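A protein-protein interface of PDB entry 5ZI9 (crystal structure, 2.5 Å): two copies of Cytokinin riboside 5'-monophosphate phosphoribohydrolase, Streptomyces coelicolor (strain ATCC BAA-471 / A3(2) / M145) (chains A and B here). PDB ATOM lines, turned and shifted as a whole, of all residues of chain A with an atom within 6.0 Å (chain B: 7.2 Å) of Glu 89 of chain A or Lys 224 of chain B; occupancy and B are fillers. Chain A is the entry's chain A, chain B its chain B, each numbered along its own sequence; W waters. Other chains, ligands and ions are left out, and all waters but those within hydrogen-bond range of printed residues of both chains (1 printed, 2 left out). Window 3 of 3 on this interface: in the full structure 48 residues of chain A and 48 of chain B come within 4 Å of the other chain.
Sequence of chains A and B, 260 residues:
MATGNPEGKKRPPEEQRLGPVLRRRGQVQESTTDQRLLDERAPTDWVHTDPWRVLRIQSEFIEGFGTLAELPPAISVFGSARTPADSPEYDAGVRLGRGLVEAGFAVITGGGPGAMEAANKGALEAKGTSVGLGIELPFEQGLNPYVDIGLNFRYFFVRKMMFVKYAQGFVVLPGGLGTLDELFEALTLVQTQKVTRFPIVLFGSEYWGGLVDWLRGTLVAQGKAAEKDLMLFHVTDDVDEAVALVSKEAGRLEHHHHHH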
ATOM      1  N   SER A  80     -15.679 -10.287  21.955  1.00  0.00           N
ATOM      2  CA  SER A  80     -16.190  -9.284  21.085  1.00  0.00           C
ATOM      3  C   SER A  80     -15.607  -7.955  21.404  1.00  0.00           C
ATOM      4  O   SER A  80     -15.603  -7.528  22.564  1.00  0.00           O
ATOM      5  CB  SER A  80     -17.702  -9.202  21.253  1.00  0.00           C
ATOM      6  OG  SER A  80     -18.291  -8.376  20.290  1.00  0.00           O
ATOM      7  N   ARG A  82     -17.102  -5.398  20.416  1.00  0.00           N
ATOM      8  CA  ARG A  82     -18.301  -4.576  20.341  1.00  0.00           C
ATOM      9  C   ARG A  82     -19.128  -4.593  21.615  1.00  0.00           C
ATOM     10  O   ARG A  82     -20.046  -3.776  21.757  1.00  0.00           O
ATOM     11  CB  ARG A  82     -19.148  -5.059  19.171  1.00  0.00           C
ATOM     12  CG  ARG A  82     -18.547  -4.685  17.817  1.00  0.00           C
ATOM     13  CD  ARG A  82     -18.983  -5.654  16.728  1.00  0.00           C
ATOM     14  NE  ARG A  82     -18.117  -5.630  15.545  1.00  0.00           N
ATOM     15  CZ  ARG A  82     -18.495  -5.915  14.290  1.00  0.00           C
ATOM     16  NH1 ARG A  82     -19.758  -6.207  13.997  1.00  0.00           N
ATOM     17  NH2 ARG A  82     -17.601  -5.893  13.300  1.00  0.00           N
ATOM     18  N   THR A  83     -18.828  -5.522  22.518  1.00  0.00           N
ATOM     19  CA  THR A  83     -19.562  -5.665  23.769  1.00  0.00           C
ATOM     20  C   THR A  83     -19.672  -4.300  24.479  1.00  0.00           C
ATOM     21  O   THR A  83     -18.689  -3.642  24.685  1.00  0.00           O
ATOM     22  CB  THR A  83     -18.889  -6.694  24.701  1.00  0.00           C
ATOM     23  OG1 THR A  83     -18.803  -7.941  24.017  1.00  0.00           O
ATOM     24  CG2 THR A  83     -19.690  -6.925  25.998  1.00  0.00           C
ATOM     25  N   PRO A  84     -20.897  -3.854  24.806  1.00  0.00           N
ATOM     26  CA  PRO A  84     -21.045  -2.568  25.523  1.00  0.00           C
ATOM     27  C   PRO A  84     -20.790  -2.724  27.007  1.00  0.00           C
ATOM     28  O   PRO A  84     -21.069  -3.785  27.558  1.00  0.00           O
ATOM     29  CB  PRO A  84     -22.503  -2.198  25.286  1.00  0.00           C
ATOM     30  CG  PRO A  84     -23.185  -3.484  24.972  1.00  0.00           C
ATOM     31  CD  PRO A  84     -22.192  -4.373  24.310  1.00  0.00           C
ATOM     32  N   SER A  87     -23.378  -4.081  29.547  1.00  0.00           N
ATOM     33  CA  SER A  87     -23.724  -5.495  29.398  1.00  0.00           C
ATOM     34  C   SER A  87     -23.320  -6.449  30.537  1.00  0.00           C
ATOM     35  O   SER A  87     -22.303  -6.249  31.181  1.00  0.00           O
ATOM     36  CB  SER A  87     -23.123  -6.027  28.106  1.00  0.00           C
ATOM     37  OG  SER A  87     -23.608  -7.343  27.878  1.00  0.00           O
ATOM     38  N   PRO A  88     -24.127  -7.498  30.789  1.00  0.00           N
ATOM     39  CA  PRO A  88     -23.752  -8.728  31.555  1.00  0.00           C
ATOM     40  C   PRO A  88     -22.472  -9.470  31.058  1.00  0.00           C
ATOM     41  O   PRO A  88     -21.685  -9.968  31.861  1.00  0.00           O
ATOM     42  CB  PRO A  88     -24.974  -9.659  31.378  1.00  0.00           C
ATOM     43  CG  PRO A  88     -26.067  -8.780  30.954  1.00  0.00           C
ATOM     44  CD  PRO A  88     -25.582  -7.401  30.638  1.00  0.00           C
ATOM     45  N   GLU A  89     -22.342  -9.586  29.741  1.00  0.00           N
ATOM     46  CA  GLU A  89     -21.135 -10.100  29.084  1.00  0.00           C
ATOM     47  C   GLU A  89     -19.874  -9.299  29.456  1.00  0.00           C
ATOM     48  O   GLU A  89     -18.784  -9.851  29.632  1.00  0.00           O
ATOM     49  CB  GLU A  89     -21.303 -10.064  27.559  1.00  0.00           C
ATOM     50  CG  GLU A  89     -21.932 -11.327  27.003  1.00  0.00           C
ATOM     51  CD  GLU A  89     -22.084 -11.298  25.473  1.00  0.00           C
ATOM     52  OE1 GLU A  89     -21.276 -10.630  24.743  1.00  0.00           O
ATOM     53  OE2 GLU A  89     -23.032 -11.967  25.016  1.00  0.00           O
ATOM     54  N   TYR A  90     -20.039  -7.995  29.543  1.00  0.00           N
ATOM     55  CA  TYR A  90     -18.953  -7.121  29.939  1.00  0.00           C
ATOM     56  C   TYR A  90     -18.593  -7.358  31.414  1.00  0.00           C
ATOM     57  O   TYR A  90     -17.415  -7.476  31.793  1.00  0.00           O
ATOM     58  CB  TYR A  90     -19.334  -5.662  29.666  1.00  0.00           C
ATOM     59  CG  TYR A  90     -18.186  -4.724  29.774  1.00  0.00           C
ATOM     60  CD1 TYR A  90     -17.750  -4.299  31.012  1.00  0.00           C
ATOM     61  CD2 TYR A  90     -17.513  -4.250  28.649  1.00  0.00           C
ATOM     62  CE1 TYR A  90     -16.703  -3.420  31.158  1.00  0.00           C
ATOM     63  CE2 TYR A  90     -16.446  -3.375  28.782  1.00  0.00           C
ATOM     64  CZ  TYR A  90     -16.060  -2.964  30.058  1.00  0.00           C
ATOM     65  OH  TYR A  90     -15.014  -2.094  30.283  1.00  0.00           O
ATOM     66  N   ASP A  91     -19.613  -7.442  32.245  1.00  0.00           N
ATOM     67  CA  ASP A  91     -19.415  -7.715  33.644  1.00  0.00           C
ATOM     68  C   ASP A  91     -18.679  -9.068  33.864  1.00  0.00           C
ATOM     69  O   ASP A  91     -17.777  -9.166  34.670  1.00  0.00           O
ATOM     70  CB  ASP A  91     -20.768  -7.682  34.354  1.00  0.00           C
ATOM     71  CG  ASP A  91     -20.609  -7.747  35.822  1.00  0.00           C
ATOM     72  OD1 ASP A  91     -20.048  -6.763  36.380  1.00  0.00           O
ATOM     73  OD2 ASP A  91     -20.970  -8.798  36.406  1.00  0.00           O
ATOM     74  N   ALA A  92     -19.067 -10.087  33.100  1.00  0.00           N
ATOM     75  CA  ALA A  92     -18.427 -11.407  33.094  1.00  0.00           C
ATOM     76  C   ALA A  92     -16.955 -11.310  32.775  1.00  0.00           C
ATOM     77  O   ALA A  92     -16.152 -11.962  33.404  1.00  0.00           O
ATOM     78  CB  ALA A  92     -19.107 -12.310  32.093  1.00  0.00           C
ATOM     79  N   GLY A  93     -16.588 -10.481  31.812  1.00  0.00           N
ATOM     80  CA  GLY A  93     -15.171 -10.280  31.480  1.00  0.00           C
ATOM     81  C   GLY A  93     -14.427  -9.573  32.596  1.00  0.00           C
ATOM     82  O   GLY A  93     -13.301  -9.926  32.908  1.00  0.00           O
ATOM     83  N   VAL A  94     -15.060  -8.581  33.215  1.00  0.00           N
ATOM     84  CA  VAL A  94     -14.445  -7.963  34.387  1.00  0.00           C
ATOM     85  C   VAL A  94     -14.256  -9.005  35.498  1.00  0.00           C
ATOM     86  O   VAL A  94     -13.207  -9.068  36.147  1.00  0.00           O
ATOM     87  CB  VAL A  94     -15.250  -6.791  34.933  1.00  0.00           C
ATOM     88  CG1 VAL A  94     -14.482  -6.130  36.087  1.00  0.00           C
ATOM     89  CG2 VAL A  94     -15.533  -5.773  33.822  1.00  0.00           C
ATOM     90  N   ALA A 115     -15.258  -6.852  25.383  1.00  0.00           N
ATOM     91  CA  ALA A 115     -14.719  -7.945  26.185  1.00  0.00           C
ATOM     92  C   ALA A 115     -13.208  -7.873  26.481  1.00  0.00           C
ATOM     93  O   ALA A 115     -12.807  -8.266  27.562  1.00  0.00           O
ATOM     94  CB  ALA A 115     -15.044  -9.271  25.525  1.00  0.00           C
ATOM     95  N   ALA A 118     -12.898  -5.272  29.129  1.00  0.00           N
ATOM     96  CA  ALA A 118     -13.467  -5.790  30.351  1.00  0.00           C
ATOM     97  C   ALA A 118     -12.473  -6.656  31.149  1.00  0.00           C
ATOM     98  O   ALA A 118     -12.359  -6.526  32.358  1.00  0.00           O
ATOM     99  CB  ALA A 118     -14.718  -6.603  30.038  1.00  0.00           C
ATOM    100  N   LEU A 173     -14.669 -15.493  25.514  1.00  0.00           N
ATOM    101  CA  LEU A 173     -15.971 -14.847  25.743  1.00  0.00           C
ATOM    102  C   LEU A 173     -16.695 -14.718  24.427  1.00  0.00           C
ATOM    103  O   LEU A 173     -16.043 -14.661  23.376  1.00  0.00           O
ATOM    104  CB  LEU A 173     -15.804 -13.465  26.340  1.00  0.00           C
ATOM    105  CG  LEU A 173     -15.025 -13.460  27.657  1.00  0.00           C
ATOM    106  CD1 LEU A 173     -14.505 -12.073  27.982  1.00  0.00           C
ATOM    107  CD2 LEU A 173     -15.895 -13.945  28.804  1.00  0.00           C
ATOM    108  N   PRO A 174     -18.043 -14.654  24.471  1.00  0.00           N
ATOM    109  CA  PRO A 174     -18.826 -14.518  23.239  1.00  0.00           C
ATOM    110  C   PRO A 174     -18.226 -13.454  22.359  1.00  0.00           C
ATOM    111  O   PRO A 174     -17.930 -12.360  22.855  1.00  0.00           O
ATOM    112  CB  PRO A 174     -20.210 -14.134  23.753  1.00  0.00           C
ATOM    113  CG  PRO A 174     -20.296 -14.829  25.062  1.00  0.00           C
ATOM    114  CD  PRO A 174     -18.926 -14.696  25.655  1.00  0.00           C
ATOM    115  N   GLY A 175     -17.962 -13.818  21.099  1.00  0.00           N
ATOM    116  CA  GLY A 175     -17.253 -12.937  20.188  1.00  0.00           C
ATOM    117  C   GLY A 175     -17.502 -13.201  18.739  1.00  0.00           C
ATOM    118  O   GLY A 175     -18.270 -14.097  18.357  1.00  0.00           O
ATOM    119  N   GLY A 176     -16.818 -12.398  17.944  1.00  0.00           N
ATOM    120  CA  GLY A 176     -16.975 -12.407  16.502  1.00  0.00           C
ATOM    121  C   GLY A 176     -15.998 -13.243  15.706  1.00  0.00           C
ATOM    122  O   GLY A 176     -15.500 -14.255  16.173  1.00  0.00           O
ATOM    123  N   LEU A 177     -15.717 -12.773  14.494  1.00  0.00           N
ATOM    124  CA  LEU A 177     -14.868 -13.491  13.557  1.00  0.00           C
ATOM    125  C   LEU A 177     -13.452 -13.660  14.106  1.00  0.00           C
ATOM    126  O   LEU A 177     -12.892 -14.746  14.007  1.00  0.00           O
ATOM    127  CB  LEU A 177     -14.843 -12.795  12.191  1.00  0.00           C
ATOM    128  CG  LEU A 177     -16.218 -12.642  11.476  1.00  0.00           C
ATOM    129  CD1 LEU A 177     -16.043 -11.967  10.111  1.00  0.00           C
ATOM    130  CD2 LEU A 177     -16.996 -13.955  11.348  1.00  0.00           C
ATOM    131  N   TYR A 207     -24.692 -19.133  23.764  1.00  0.00           N
ATOM    132  CA  TYR A 207     -23.963 -18.506  22.680  1.00  0.00           C
ATOM    133  C   TYR A 207     -23.225 -19.517  21.801  1.00  0.00           C
ATOM    134  O   TYR A 207     -23.395 -19.516  20.557  1.00  0.00           O
ATOM    135  CB  TYR A 207     -22.971 -17.510  23.228  1.00  0.00           C
ATOM    136  CG  TYR A 207     -22.353 -16.725  22.122  1.00  0.00           C
ATOM    137  CD1 TYR A 207     -23.026 -15.654  21.597  1.00  0.00           C
ATOM    138  CD2 TYR A 207     -21.098 -17.062  21.578  1.00  0.00           C
ATOM    139  CE1 TYR A 207     -22.500 -14.902  20.567  1.00  0.00           C
ATOM    140  CE2 TYR A 207     -20.541 -16.325  20.548  1.00  0.00           C
ATOM    141  CZ  TYR A 207     -21.259 -15.226  20.039  1.00  0.00           C
ATOM    142  OH  TYR A 207     -20.789 -14.413  19.014  1.00  0.00           O
ATOM    143  N   GLN B 191     -12.207  -8.719   7.099  1.00  0.00           N
ATOM    144  CA  GLN B 191     -13.058  -7.861   7.922  1.00  0.00           C
ATOM    145  C   GLN B 191     -12.336  -6.644   8.482  1.00  0.00           C
ATOM    146  O   GLN B 191     -12.889  -5.578   8.544  1.00  0.00           O
ATOM    147  CB  GLN B 191     -13.643  -8.634   9.101  1.00  0.00           C
ATOM    148  CG  GLN B 191     -14.647  -7.826   9.930  1.00  0.00           C
ATOM    149  CD  GLN B 191     -15.078  -8.538  11.211  1.00  0.00           C
ATOM    150  OE1 GLN B 191     -14.232  -8.972  12.011  1.00  0.00           O
ATOM    151  NE2 GLN B 191     -16.383  -8.666  11.411  1.00  0.00           N
ATOM    152  N   THR B 218     -26.866 -16.560  15.656  1.00  0.00           N
ATOM    153  CA  THR B 218     -26.235 -16.135  16.924  1.00  0.00           C
ATOM    154  C   THR B 218     -25.323 -14.918  16.790  1.00  0.00           C
ATOM    155  O   THR B 218     -25.614 -13.935  17.447  1.00  0.00           O
ATOM    156  CB  THR B 218     -25.493 -17.286  17.567  1.00  0.00           C
ATOM    157  OG1 THR B 218     -26.409 -18.378  17.705  1.00  0.00           O
ATOM    158  CG2 THR B 218     -24.957 -16.900  18.926  1.00  0.00           C
ATOM    159  N   LEU B 219     -24.270 -14.940  15.966  1.00  0.00           N
ATOM    160  CA  LEU B 219     -23.317 -13.797  15.947  1.00  0.00           C
ATOM    161  C   LEU B 219     -23.923 -12.474  15.432  1.00  0.00           C
ATOM    162  O   LEU B 219     -23.833 -11.423  16.098  1.00  0.00           O
ATOM    163  CB  LEU B 219     -22.058 -14.017  15.084  1.00  0.00           C
ATOM    164  CG  LEU B 219     -21.005 -15.092  15.190  1.00  0.00           C
ATOM    165  CD1 LEU B 219     -19.637 -14.446  15.085  1.00  0.00           C
ATOM    166  CD2 LEU B 219     -21.117 -15.903  16.455  1.00  0.00           C
ATOM    167  N   VAL B 220     -24.470 -12.517  14.222  1.00  0.00           N
ATOM    168  CA  VAL B 220     -25.031 -11.324  13.601  1.00  0.00           C
ATOM    169  C   VAL B 220     -26.258 -10.840  14.405  1.00  0.00           C
ATOM    170  O   VAL B 220     -26.432  -9.639  14.657  1.00  0.00           O
ATOM    171  CB  VAL B 220     -25.409 -11.595  12.140  1.00  0.00           C
ATOM    172  CG1 VAL B 220     -26.091 -10.389  11.535  1.00  0.00           C
ATOM    173  CG2 VAL B 220     -24.153 -11.926  11.337  1.00  0.00           C
ATOM    174  N   ALA B 221     -27.065 -11.800  14.830  1.00  0.00           N
ATOM    175  CA  ALA B 221     -28.268 -11.520  15.541  1.00  0.00           C
ATOM    176  C   ALA B 221     -28.004 -10.846  16.891  1.00  0.00           C
ATOM    177  O   ALA B 221     -28.890 -10.186  17.408  1.00  0.00           O
ATOM    178  CB  ALA B 221     -29.028 -12.809  15.744  1.00  0.00           C
ATOM    179  N   GLN B 222     -26.813 -11.030  17.477  1.00  0.00           N
ATOM    180  CA  GLN B 222     -26.481 -10.410  18.776  1.00  0.00           C
ATOM    181  C   GLN B 222     -25.507  -9.259  18.658  1.00  0.00           C
ATOM    182  O   GLN B 222     -25.061  -8.746  19.689  1.00  0.00           O
ATOM    183  CB  GLN B 222     -25.956 -11.444  19.761  1.00  0.00           C
ATOM    184  CG  GLN B 222     -26.928 -12.589  20.031  1.00  0.00           C
ATOM    185  CD  GLN B 222     -26.417 -13.550  21.083  1.00  0.00           C
ATOM    186  OE1 GLN B 222     -25.414 -13.269  21.751  1.00  0.00           O
ATOM    187  NE2 GLN B 222     -27.115 -14.684  21.262  1.00  0.00           N
ATOM    188  N   GLY B 223     -25.173  -8.839  17.435  1.00  0.00           N
ATOM    189  CA  GLY B 223     -24.279  -7.692  17.240  1.00  0.00           C
ATOM    190  C   GLY B 223     -22.780  -7.935  17.212  1.00  0.00           C
ATOM    191  O   GLY B 223     -22.044  -6.970  17.146  1.00  0.00           O
ATOM    192  N   LYS B 224     -22.327  -9.200  17.210  1.00  0.00           N
ATOM    193  CA  LYS B 224     -20.889  -9.537  17.214  1.00  0.00           C
ATOM    194  C   LYS B 224     -20.307  -9.414  15.820  1.00  0.00           C
ATOM    195  O   LYS B 224     -19.129  -9.125  15.646  1.00  0.00           O
ATOM    196  CB  LYS B 224     -20.619 -10.944  17.726  1.00  0.00           C
ATOM    197  CG  LYS B 224     -21.497 -11.391  18.895  1.00  0.00           C
ATOM    198  CD  LYS B 224     -21.290 -10.630  20.195  1.00  0.00           C
ATOM    199  CE  LYS B 224     -21.624 -11.499  21.423  1.00  0.00           C
ATOM    200  NZ  LYS B 224     -22.982 -11.309  22.024  1.00  0.00           N
ATOM    201  N   ALA B 225     -21.137  -9.656  14.820  1.00  0.00           N
ATOM    202  CA  ALA B 225     -20.798  -9.368  13.424  1.00  0.00           C
ATOM    203  C   ALA B 225     -21.953  -8.586  12.789  1.00  0.00           C
ATOM    204  O   ALA B 225     -23.078  -8.523  13.336  1.00  0.00           O
ATOM    205  CB  ALA B 225     -20.555 -10.663  12.669  1.00  0.00           C
ATOM    206  N   ALA B 226     -21.663  -7.993  11.636  1.00  0.00           N
ATOM    207  CA  ALA B 226     -22.676  -7.321  10.823  1.00  0.00           C
ATOM    208  C   ALA B 226     -23.171  -8.303   9.768  1.00  0.00           C
ATOM    209  O   ALA B 226     -22.454  -9.248   9.410  1.00  0.00           O
ATOM    210  CB  ALA B 226     -22.066  -6.087  10.167  1.00  0.00           C
ATOM    211  N   ASP B 229     -20.838  -8.682   6.891  1.00  0.00           N
ATOM    212  CA  ASP B 229     -19.635  -9.494   7.185  1.00  0.00           C
ATOM    213  C   ASP B 229     -19.761 -10.937   6.661  1.00  0.00           C
ATOM    214  O   ASP B 229     -18.745 -11.604   6.416  1.00  0.00           O
ATOM    215  CB  ASP B 229     -19.304  -9.515   8.702  1.00  0.00           C
ATOM    216  CG  ASP B 229     -18.798  -8.159   9.243  1.00  0.00           C
ATOM    217  OD1 ASP B 229     -18.154  -7.360   8.527  1.00  0.00           O
ATOM    218  OD2 ASP B 229     -19.047  -7.873  10.421  1.00  0.00           O
HETATM  219  O   HOH W   1     -26.026 -20.818  19.701  1.00  0.00           O
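NH1 of Arg 82 of chain A is in hydrogen-bond range of O of Lys 224 of chain B, 3.4 Å away.
The guanidinium group of Arg 82 of chain A is in salt-bridge range of the side-chain carboxylate of Asp 229 of chain B.
The side-chain carboxylate of Glu 89 of chain A lies within salt-bridge range of the side-chain amino group of Lys 224 of chain B.
The backbone NH (N) of Arg 82 of chain A sits close to the side-chain hydroxyl (OG) of Ser 80 of chain A (3.2 Å).
The backbone carbonyl oxygen (O) of Ser 80 of chain A is in hydrogen-bond range of the backbone NH (N) of Ala 115 of chain A, at 2.9 Å.
The backbone carbonyl oxygen (O) of Pro 174 of chain A is in hydrogen-bond range of the backbone NH (N) of Ser 80 of chain A, at 3.2 Å.
OH of Tyr 207 of chain A is in hydrogen-bond range of O of Gly 175 of chain A (2.6 Å).
The backbone NH (N) of Ala 225 of chain B sits at hydrogen-bond distance from the backbone carbonyl oxygen (O) of Leu 219 of chain B, 3.5 Å away.
The side-chain amide oxygen of Gln 222 of chain B is in hydrogen-bond range of the side-chain amino group of Lys 224 of chain B (3.1 Å).
Among the printed residues, pairs that only touch across the chains: Ser 80 of chain A with Lys 224 of chain B (3.8 Å), Arg 82 of chain A with Gln 191 of chain B (3.6 Å), Arg 82 of chain A with Gly 223 of chain B (3.4 Å), Arg 82 of chain A with Ala 225 of chain B (3.4 Å), Arg 82 of chain A with Ala 226 of chain B (3.5 Å), Pro 174 of chain A with Lys 224 of chain B (3.8 Å), Gly 175 of chain A with Leu 219 of chain B (3.6 Å), Gly 175 of chain A with Lys 224 of chain B (3.98 Å), Gly 176 of chain A with Leu 219 of chain B (3.6 Å), Leu 177 of chain A with Gln 191 of chain B (3.6 Å), Tyr 207 of chain A with Thr 218 of chain B (3.5 Å), Tyr 207 of chain A with Leu 219 of chain B (3.0 Å), Tyr 207 of chain A with Gln 222 of chain B (3.4 Å) and Tyr 207 of chain A with Lys 224 of chain B (3.1 Å).
Of chain B, only Lys 224 (3.1 Å) comes within 4 Å of Glu 89 of chain A.
Of the printed residues of chain A, Lys 224 of chain B touches Ser 80 (3.8 Å), Arg 82 (3.4 Å), Glu 89 (3.1 Å), Pro 174 (3.8 Å), Gly 175 (3.98 Å) and Tyr 207 (3.1 Å).
Of the printed residues of chain B, Gly 176 of chain A touches Leu 219 (3.6 Å).
Of the printed residues of chain A, Gly 223 of chain B touches Arg 82 (3.4 Å).
Hydrophobic or aromatic side chains of chain B within 4 Å of the printed part of chain A: Leu 219.
Of the 20 printed residues of chain A, 8 touch a printed residue of chain B.
Printed residues of chain A that touch a printed residue of chain B: Ser 80, Arg 82, Glu 89, Pro 174, Gly 175, Gly 176, Leu 177 and Tyr 207.
Hydrophobic or aromatic side chains of chain A that line the printed part of chain B: Pro 174, Leu 177 and Tyr 207.
Among the printed residues, 17 pairs touch across the chains.
No position is printed for both chains.
Of the 17 pairs that touch across the chains among the printed residues, none has its exchanged pair printed and touching as well.
Water W1 bridges the backbone carbonyl oxygen of Tyr 207 of chain A (3.1 Å) and the side-chain hydroxyl of Thr 218 of chain B (3.2 Å).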
